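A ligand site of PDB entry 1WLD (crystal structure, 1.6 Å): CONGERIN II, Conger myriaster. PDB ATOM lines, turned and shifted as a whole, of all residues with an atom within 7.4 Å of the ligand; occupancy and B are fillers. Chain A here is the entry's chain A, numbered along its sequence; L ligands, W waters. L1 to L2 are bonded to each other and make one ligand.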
ATOM      1  N   ARG A  29     -16.090   7.783  11.170  1.00  0.00           N
ATOM      2  CA  ARG A  29     -14.886   8.181  10.480  1.00  0.00           C
ATOM      3  C   ARG A  29     -13.654   7.909  11.358  1.00  0.00           C
ATOM      4  O   ARG A  29     -13.789   7.929  12.592  1.00  0.00           O
ATOM      5  CB  ARG A  29     -14.959   9.696  10.109  1.00  0.00           C
ATOM      6  CG  ARG A  29     -15.226  10.530  11.357  1.00  0.00           C
ATOM      7  CD  ARG A  29     -15.647  11.965  11.134  1.00  0.00           C
ATOM      8  NE  ARG A  29     -14.549  12.763  10.640  1.00  0.00           N
ATOM      9  CZ  ARG A  29     -14.008  13.858  11.138  1.00  0.00           C
ATOM     10  NH1 ARG A  29     -14.346  14.493  12.244  1.00  0.00           N
ATOM     11  NH2 ARG A  29     -12.993  14.397  10.463  1.00  0.00           N
ATOM     12  N   SER A  31      -9.119   8.788  11.067  1.00  0.00           N
ATOM     13  CA  SER A  31      -8.088   9.362  10.168  1.00  0.00           C
ATOM     14  C   SER A  31      -6.708   8.806  10.495  1.00  0.00           C
ATOM     15  O   SER A  31      -6.474   8.391  11.633  1.00  0.00           O
ATOM     16  CB  SER A  31      -8.095  10.896  10.312  1.00  0.00           C
ATOM     17  OG  SER A  31      -7.782  11.263  11.656  1.00  0.00           O
ATOM     18  N   ASN A  33      -2.754  10.287  10.332  1.00  0.00           N
ATOM     19  CA  ASN A  33      -2.219  11.649  10.316  1.00  0.00           C
ATOM     20  C   ASN A  33      -0.694  11.645  10.412  1.00  0.00           C
ATOM     21  O   ASN A  33      -0.174  10.905  11.246  1.00  0.00           O
ATOM     22  CB  ASN A  33      -2.727  12.443  11.545  1.00  0.00           C
ATOM     23  CG  ASN A  33      -4.245  12.514  11.554  1.00  0.00           C
ATOM     24  OD1 ASN A  33      -4.804  13.426  10.940  1.00  0.00           O
ATOM     25  ND2 ASN A  33      -4.919  11.545  12.190  1.00  0.00           N
ATOM     26  N   HIS A  44      -3.304  14.592   6.511  1.00  0.00           N
ATOM     27  CA  HIS A  44      -4.449  14.006   7.168  1.00  0.00           C
ATOM     28  C   HIS A  44      -5.286  13.250   6.157  1.00  0.00           C
ATOM     29  O   HIS A  44      -5.677  13.860   5.151  1.00  0.00           O
ATOM     30  CB  HIS A  44      -5.292  15.110   7.799  1.00  0.00           C
ATOM     31  CG  HIS A  44      -6.668  14.828   8.257  1.00  0.00           C
ATOM     32  ND1 HIS A  44      -6.950  14.218   9.462  1.00  0.00           N
ATOM     33  CD2 HIS A  44      -7.874  15.125   7.689  1.00  0.00           C
ATOM     34  CE1 HIS A  44      -8.267  14.165   9.616  1.00  0.00           C
ATOM     35  NE2 HIS A  44      -8.850  14.682   8.560  1.00  0.00           N
ATOM     36  N   MET A  45      -5.545  11.976   6.406  1.00  0.00           N
ATOM     37  CA  MET A  45      -6.402  11.211   5.492  1.00  0.00           C
ATOM     38  C   MET A  45      -7.574  10.660   6.294  1.00  0.00           C
ATOM     39  O   MET A  45      -7.383   9.782   7.141  1.00  0.00           O
ATOM     40  CB  MET A  45      -5.653  10.052   4.823  1.00  0.00           C
ATOM     41  CG  MET A  45      -6.625   9.302   3.887  1.00  0.00           C
ATOM     42  SD  MET A  45      -5.850   8.151   2.725  1.00  0.00           S
ATOM     43  CE  MET A  45      -4.880   7.262   3.981  1.00  0.00           C
ATOM     44  N   ASP A  46      -8.770  11.184   6.038  1.00  0.00           N
ATOM     45  CA  ASP A  46      -9.939  10.847   6.819  1.00  0.00           C
ATOM     46  C   ASP A  46     -10.771   9.827   6.037  1.00  0.00           C
ATOM     47  O   ASP A  46     -10.991  10.012   4.837  1.00  0.00           O
ATOM     48  CB  ASP A  46     -10.749  12.130   7.124  1.00  0.00           C
ATOM     49  CG  ASP A  46     -11.737  11.973   8.246  1.00  0.00           C
ATOM     50  OD1 ASP A  46     -11.582  11.036   9.074  1.00  0.00           O
ATOM     51  OD2 ASP A  46     -12.718  12.754   8.287  1.00  0.00           O
ATOM     52  N   ARG A  48     -14.303   8.428   5.760  1.00  0.00           N
ATOM     53  CA  ARG A  48     -15.627   8.825   6.198  1.00  0.00           C
ATOM     54  C   ARG A  48     -16.691   7.807   5.786  1.00  0.00           C
ATOM     55  O   ARG A  48     -16.969   7.690   4.602  1.00  0.00           O
ATOM     56  CB  ARG A  48     -15.951  10.220   5.638  1.00  0.00           C
ATOM     57  CG  ARG A  48     -14.975  11.272   6.202  1.00  0.00           C
ATOM     58  CD  ARG A  48     -15.251  12.652   5.593  1.00  0.00           C
ATOM     59  NE  ARG A  48     -14.326  13.629   6.214  1.00  0.00           N
ATOM     60  CZ  ARG A  48     -14.380  14.939   6.079  1.00  0.00           C
ATOM     61  NH1 ARG A  48     -15.371  15.424   5.309  1.00  0.00           N
ATOM     62  NH2 ARG A  48     -13.522  15.750   6.675  1.00  0.00           N
ATOM     63  N   TYR A  51     -20.385  11.019   7.576  1.00  0.00           N
ATOM     64  CA  TYR A  51     -19.976  12.293   8.191  1.00  0.00           C
ATOM     65  C   TYR A  51     -20.603  13.444   7.401  1.00  0.00           C
ATOM     66  O   TYR A  51     -20.188  13.762   6.286  1.00  0.00           O
ATOM     67  CB  TYR A  51     -18.465  12.432   8.225  1.00  0.00           C
ATOM     68  CG  TYR A  51     -17.930  13.703   8.847  1.00  0.00           C
ATOM     69  CD1 TYR A  51     -18.138  13.963  10.182  1.00  0.00           C
ATOM     70  CD2 TYR A  51     -17.261  14.654   8.088  1.00  0.00           C
ATOM     71  CE1 TYR A  51     -17.667  15.118  10.790  1.00  0.00           C
ATOM     72  CE2 TYR A  51     -16.790  15.828   8.664  1.00  0.00           C
ATOM     73  CZ  TYR A  51     -16.987  16.036  10.017  1.00  0.00           C
ATOM     74  OH  TYR A  51     -16.540  17.207  10.598  1.00  0.00           O
ATOM     75  N   ALA A  53     -22.548  15.085   4.871  1.00  0.00           N
ATOM     76  CA  ALA A  53     -22.955  14.646   3.551  1.00  0.00           C
ATOM     77  C   ALA A  53     -22.013  13.628   2.914  1.00  0.00           C
ATOM     78  O   ALA A  53     -22.271  13.114   1.826  1.00  0.00           O
ATOM     79  CB  ALA A  53     -22.995  15.852   2.595  1.00  0.00           C
ATOM     80  N   ASP A  54     -20.878  13.367   3.564  1.00  0.00           N
ATOM     81  CA  ASP A  54     -19.894  12.427   3.068  1.00  0.00           C
ATOM     82  C   ASP A  54     -20.190  11.000   3.518  1.00  0.00           C
ATOM     83  O   ASP A  54     -20.207  10.704   4.710  1.00  0.00           O
ATOM     84  CB  ASP A  54     -18.499  12.812   3.588  1.00  0.00           C
ATOM     85  CG  ASP A  54     -18.030  14.128   2.999  1.00  0.00           C
ATOM     86  OD1 ASP A  54     -18.320  14.347   1.807  1.00  0.00           O
ATOM     87  OD2 ASP A  54     -17.359  14.928   3.674  1.00  0.00           O
ATOM     88  N   VAL A  59     -11.152  11.869   2.541  1.00  0.00           N
ATOM     89  CA  VAL A  59     -10.922  13.321   2.479  1.00  0.00           C
ATOM     90  C   VAL A  59      -9.516  13.612   3.007  1.00  0.00           C
ATOM     91  O   VAL A  59      -9.224  13.168   4.137  1.00  0.00           O
ATOM     92  CB  VAL A  59     -11.962  14.101   3.303  1.00  0.00           C
ATOM     93  CG1 VAL A  59     -11.668  15.587   3.234  1.00  0.00           C
ATOM     94  CG2 VAL A  59     -13.376  13.831   2.750  1.00  0.00           C
ATOM     95  N   LEU A  60      -8.684  14.221   2.197  1.00  0.00           N
ATOM     96  CA  LEU A  60      -7.301  14.502   2.595  1.00  0.00           C
ATOM     97  C   LEU A  60      -7.052  15.998   2.743  1.00  0.00           C
ATOM     98  O   LEU A  60      -7.587  16.844   1.984  1.00  0.00           O
ATOM     99  CB  LEU A  60      -6.334  13.943   1.546  1.00  0.00           C
ATOM    100  CG  LEU A  60      -6.361  12.420   1.408  1.00  0.00           C
ATOM    101  CD1 LEU A  60      -7.404  11.987   0.373  1.00  0.00           C
ATOM    102  CD2 LEU A  60      -4.991  11.924   0.988  1.00  0.00           C
ATOM    103  N   ASN A  61      -6.207  16.381   3.702  1.00  0.00           N
ATOM    104  CA  ASN A  61      -5.959  17.831   3.897  1.00  0.00           C
ATOM    105  C   ASN A  61      -4.732  18.000   4.778  1.00  0.00           C
ATOM    106  O   ASN A  61      -4.159  17.013   5.207  1.00  0.00           O
ATOM    107  CB  ASN A  61      -7.188  18.496   4.512  1.00  0.00           C
ATOM    108  CG  ASN A  61      -7.285  19.991   4.206  1.00  0.00           C
ATOM    109  OD1 ASN A  61      -6.310  20.554   3.693  1.00  0.00           O
ATOM    110  ND2 ASN A  61      -8.430  20.622   4.485  1.00  0.00           N
ATOM    111  N   SER A  62      -4.305  19.240   4.941  1.00  0.00           N
ATOM    112  CA  SER A  62      -3.252  19.594   5.893  1.00  0.00           C
ATOM    113  C   SER A  62      -3.824  20.554   6.928  1.00  0.00           C
ATOM    114  O   SER A  62      -4.753  21.316   6.655  1.00  0.00           O
ATOM    115  CB  SER A  62      -2.035  20.211   5.192  1.00  0.00           C
ATOM    116  OG  SER A  62      -2.479  21.286   4.359  1.00  0.00           O
ATOM    117  N   TRP A  69      -7.499  24.229   8.729  1.00  0.00           N
ATOM    118  CA  TRP A  69      -7.480  23.318   7.603  1.00  0.00           C
ATOM    119  C   TRP A  69      -7.325  24.090   6.299  1.00  0.00           C
ATOM    120  O   TRP A  69      -7.873  25.201   6.137  1.00  0.00           O
ATOM    121  CB  TRP A  69      -8.746  22.468   7.591  1.00  0.00           C
ATOM    122  CG  TRP A  69      -8.784  21.535   8.772  1.00  0.00           C
ATOM    123  CD1 TRP A  69      -9.488  21.664   9.921  1.00  0.00           C
ATOM    124  CD2 TRP A  69      -8.021  20.312   8.901  1.00  0.00           C
ATOM    125  NE1 TRP A  69      -9.247  20.614  10.767  1.00  0.00           N
ATOM    126  CE2 TRP A  69      -8.344  19.779  10.157  1.00  0.00           C
ATOM    127  CE3 TRP A  69      -7.134  19.627   8.091  1.00  0.00           C
ATOM    128  CZ2 TRP A  69      -7.802  18.563  10.622  1.00  0.00           C
ATOM    129  CZ3 TRP A  69      -6.568  18.437   8.550  1.00  0.00           C
ATOM    130  CH2 TRP A  69      -6.920  17.926   9.801  1.00  0.00           C
ATOM    131  N   GLN A  70      -6.513  23.527   5.423  1.00  0.00           N
ATOM    132  CA  GLN A  70      -6.257  24.102   4.105  1.00  0.00           C
ATOM    133  C   GLN A  70      -7.245  23.550   3.068  1.00  0.00           C
ATOM    134  O   GLN A  70      -8.386  23.267   3.427  1.00  0.00           O
ATOM    135  CB  GLN A  70      -4.785  23.888   3.764  1.00  0.00           C
ATOM    136  CG  GLN A  70      -3.844  24.498   4.846  1.00  0.00           C
ATOM    137  CD  GLN A  70      -4.169  25.971   5.066  1.00  0.00           C
ATOM    138  OE1 GLN A  70      -4.077  26.734   4.112  1.00  0.00           O
ATOM    139  NE2 GLN A  70      -4.540  26.396   6.263  1.00  0.00           N
ATOM    140  N   GLN A  71      -6.781  23.399   1.838  1.00  0.00           N
ATOM    141  CA  GLN A  71      -7.684  22.994   0.758  1.00  0.00           C
ATOM    142  C   GLN A  71      -7.843  21.468   0.759  1.00  0.00           C
ATOM    143  O   GLN A  71      -6.866  20.748   0.542  1.00  0.00           O
ATOM    144  CB  GLN A  71      -7.160  23.478  -0.583  1.00  0.00           C
ATOM    145  CG  GLN A  71      -7.852  22.881  -1.796  1.00  0.00           C
ATOM    146  CD  GLN A  71      -9.274  23.373  -1.923  1.00  0.00           C
ATOM    147  OE1 GLN A  71      -9.474  24.589  -2.118  1.00  0.00           O
ATOM    148  NE2 GLN A  71     -10.247  22.466  -1.830  1.00  0.00           N
ATOM    149  N   GLU A  72      -9.086  21.019   0.935  1.00  0.00           N
ATOM    150  CA  GLU A  72      -9.339  19.582   0.896  1.00  0.00           C
ATOM    151  C   GLU A  72      -9.195  18.977  -0.501  1.00  0.00           C
ATOM    152  O   GLU A  72      -9.567  19.579  -1.499  1.00  0.00           O
ATOM    153  CB  GLU A  72     -10.790  19.257   1.291  1.00  0.00           C
ATOM    154  CG  GLU A  72     -11.101  19.467   2.743  1.00  0.00           C
ATOM    155  CD  GLU A  72     -12.512  19.042   3.089  1.00  0.00           C
ATOM    156  OE1 GLU A  72     -13.363  18.728   2.205  1.00  0.00           O
ATOM    157  OE2 GLU A  72     -12.754  19.077   4.293  1.00  0.00           O
ATOM    158  N   GLU A  73      -8.762  17.729  -0.523  1.00  0.00           N
ATOM    159  CA  GLU A  73      -8.770  16.864  -1.700  1.00  0.00           C
ATOM    160  C   GLU A  73      -9.618  15.651  -1.345  1.00  0.00           C
ATOM    161  O   GLU A  73      -9.702  15.234  -0.182  1.00  0.00           O
ATOM    162  CB  GLU A  73      -7.350  16.466  -2.105  1.00  0.00           C
ATOM    163  CG  GLU A  73      -6.517  17.654  -2.548  1.00  0.00           C
ATOM    164  CD  GLU A  73      -5.258  17.354  -3.291  1.00  0.00           C
ATOM    165  OE1 GLU A  73      -4.637  18.328  -3.793  1.00  0.00           O
ATOM    166  OE2 GLU A  73      -4.782  16.215  -3.443  1.00  0.00           O
ATOM    167  N   ARG A  74     -10.382  15.140  -2.304  1.00  0.00           N
ATOM    168  CA  ARG A  74     -11.218  13.979  -2.031  1.00  0.00           C
ATOM    169  C   ARG A  74     -10.913  12.828  -2.980  1.00  0.00           C
ATOM    170  O   ARG A  74     -10.428  13.009  -4.091  1.00  0.00           O
ATOM    171  CB  ARG A  74     -12.695  14.402  -2.152  1.00  0.00           C
ATOM    172  CG  ARG A  74     -13.046  15.312  -0.988  1.00  0.00           C
ATOM    173  CD  ARG A  74     -14.454  15.867  -1.004  1.00  0.00           C
ATOM    174  NE  ARG A  74     -14.625  16.598   0.289  1.00  0.00           N
ATOM    175  CZ  ARG A  74     -15.662  16.293   1.063  1.00  0.00           C
ATOM    176  NH1 ARG A  74     -16.475  15.362   0.604  1.00  0.00           N
ATOM    177  NH2 ARG A  74     -15.831  16.919   2.220  1.00  0.00           N
HETATM  178  C1  LIG L   1     -16.205  20.257   4.943  1.00  0.00           C
HETATM  179  C2  LIG L   1     -15.667  19.199   5.907  1.00  0.00           C
HETATM  180  C3  LIG L   1     -14.902  19.869   7.043  1.00  0.00           C
HETATM  181  C4  LIG L   1     -15.832  20.901   7.692  1.00  0.00           C
HETATM  182  C5  LIG L   1     -15.221  21.680   8.794  1.00  0.00           C
HETATM  183  C6  LIG L   1     -17.066  21.217   5.720  1.00  0.00           C
HETATM  184  O1  LIG L   1     -17.256  22.331   4.580  1.00  0.00           O
HETATM  185  O2  LIG L   1     -16.997  19.584   3.971  1.00  0.00           O
HETATM  186  O3  LIG L   1     -14.864  18.293   5.210  1.00  0.00           O
HETATM  187  O4  LIG L   1     -14.618  18.900   8.016  1.00  0.00           O
HETATM  188  O5  LIG L   1     -16.220  21.868   6.663  1.00  0.00           O
HETATM  189  O6  LIG L   1     -13.941  22.241   8.482  1.00  0.00           O
HETATM  190  C1  LG2 L   2     -13.278  18.882   8.477  1.00  0.00           C
HETATM  191  C2  LG2 L   2     -13.239  17.892   9.645  1.00  0.00           C
HETATM  192  C3  LG2 L   2     -11.934  17.796  10.076  1.00  0.00           C
HETATM  193  C4  LG2 L   2     -10.920  17.280   8.969  1.00  0.00           C
HETATM  194  C5  LG2 L   2     -11.095  18.271   7.815  1.00  0.00           C
HETATM  195  C6  LG2 L   2     -10.341  17.881   6.557  1.00  0.00           C
HETATM  196  O1  LG2 L   2     -14.023  18.415  10.705  1.00  0.00           O
HETATM  197  O2  LG2 L   2     -11.746  16.904  11.247  1.00  0.00           O
HETATM  198  O3  LG2 L   2     -11.277  15.953   8.594  1.00  0.00           O
HETATM  199  O4  LG2 L   2     -12.480  18.354   7.417  1.00  0.00           O
HETATM  200  O5  LG2 L   2     -10.426  18.983   5.638  1.00  0.00           O
HETATM  201  O   HOH W   1     -14.967  23.757   3.773  1.00  0.00           O
HETATM  202  O   HOH W   2     -13.712  16.854  13.593  1.00  0.00           O
HETATM  203  O   HOH W   3     -13.782  20.606  12.418  1.00  0.00           O
HETATM  204  O   HOH W   4     -11.791  21.689   5.812  1.00  0.00           O
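The side-chain carboxylate (OE2) of Glu 72 sits at hydrogen-bond distance from an oxygen (O3) of LIG L1, 2.4 Å away.
A ring nitrogen (NE2) of His 44 is in hydrogen-bond range of an oxygen (O3) of LG2 L2.
OH of Tyr 51 is in hydrogen-bond range of O1 of LG2 L2 (2.8 Å).
The side-chain amide nitrogen (ND2) of Asn 61 is in hydrogen-bond range of an oxygen (O5) of LG2 L2.
An oxygen (O4) of LG2 L2 is in hydrogen-bond range of the guanidinium group (NH2) of Arg 48.
The guanidinium group (NH2) of Arg 29 sits at hydrogen-bond distance from an oxygen (O2) of LG2 L2 (2.9 Å).
An oxygen (O2) of LIG L1 lies within hydrogen-bond range of the guanidinium group of Arg 74 (3.4 Å).
The guanidinium group (NH2) of Arg 74 lies within salt-bridge range of the side-chain carboxylate (OE1) of Glu 72.
The backbone carbonyl oxygen (O) of Asn 61 lies within hydrogen-bond range of the backbone NH (N) of His 44 (2.9 Å).
A ring nitrogen (ND1) of His 44 is in hydrogen-bond range of the side-chain amide oxygen of Asn 33 (2.7 Å).
The side-chain amide nitrogen (ND2) of Asn 61 lies within hydrogen-bond range of the backbone carbonyl oxygen (O) of Gln 70, at 2.8 Å.
OD1 of Asn 61 sits close to O of Gln 71 (3.2 Å).
The side-chain carboxylate of Asp 46 is in salt-bridge range of the guanidinium group of Arg 48 (2.8 Å).
The guanidinium group (NH2) of Arg 29 lies within salt-bridge range of the side-chain carboxylate (OD2) of Asp 46, 2.7 Å away.
N of Asp 46 sits at hydrogen-bond distance from O of Val 59 (2.8 Å).
Asp 46 touches the ligand.
CZ2 of Trp 69 touches C4 of LG2 L2, at 3.8 Å.
Hydrophobic or aromatic side chains that line the ligand: His 44, Tyr 51 and Trp 69.
Of the 20 residues printed, 9 come within 4 Å of the ligand.
Water W4 bridges an oxygen (O5) of LG2 L2 and the side-chain carboxylate (OE2) of Glu 72.
Water W2 bridges the guanidinium group (NH1) of Arg 29 (2.8 Å) and an oxygen (O2) of LG2 L2 (3.1 Å).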
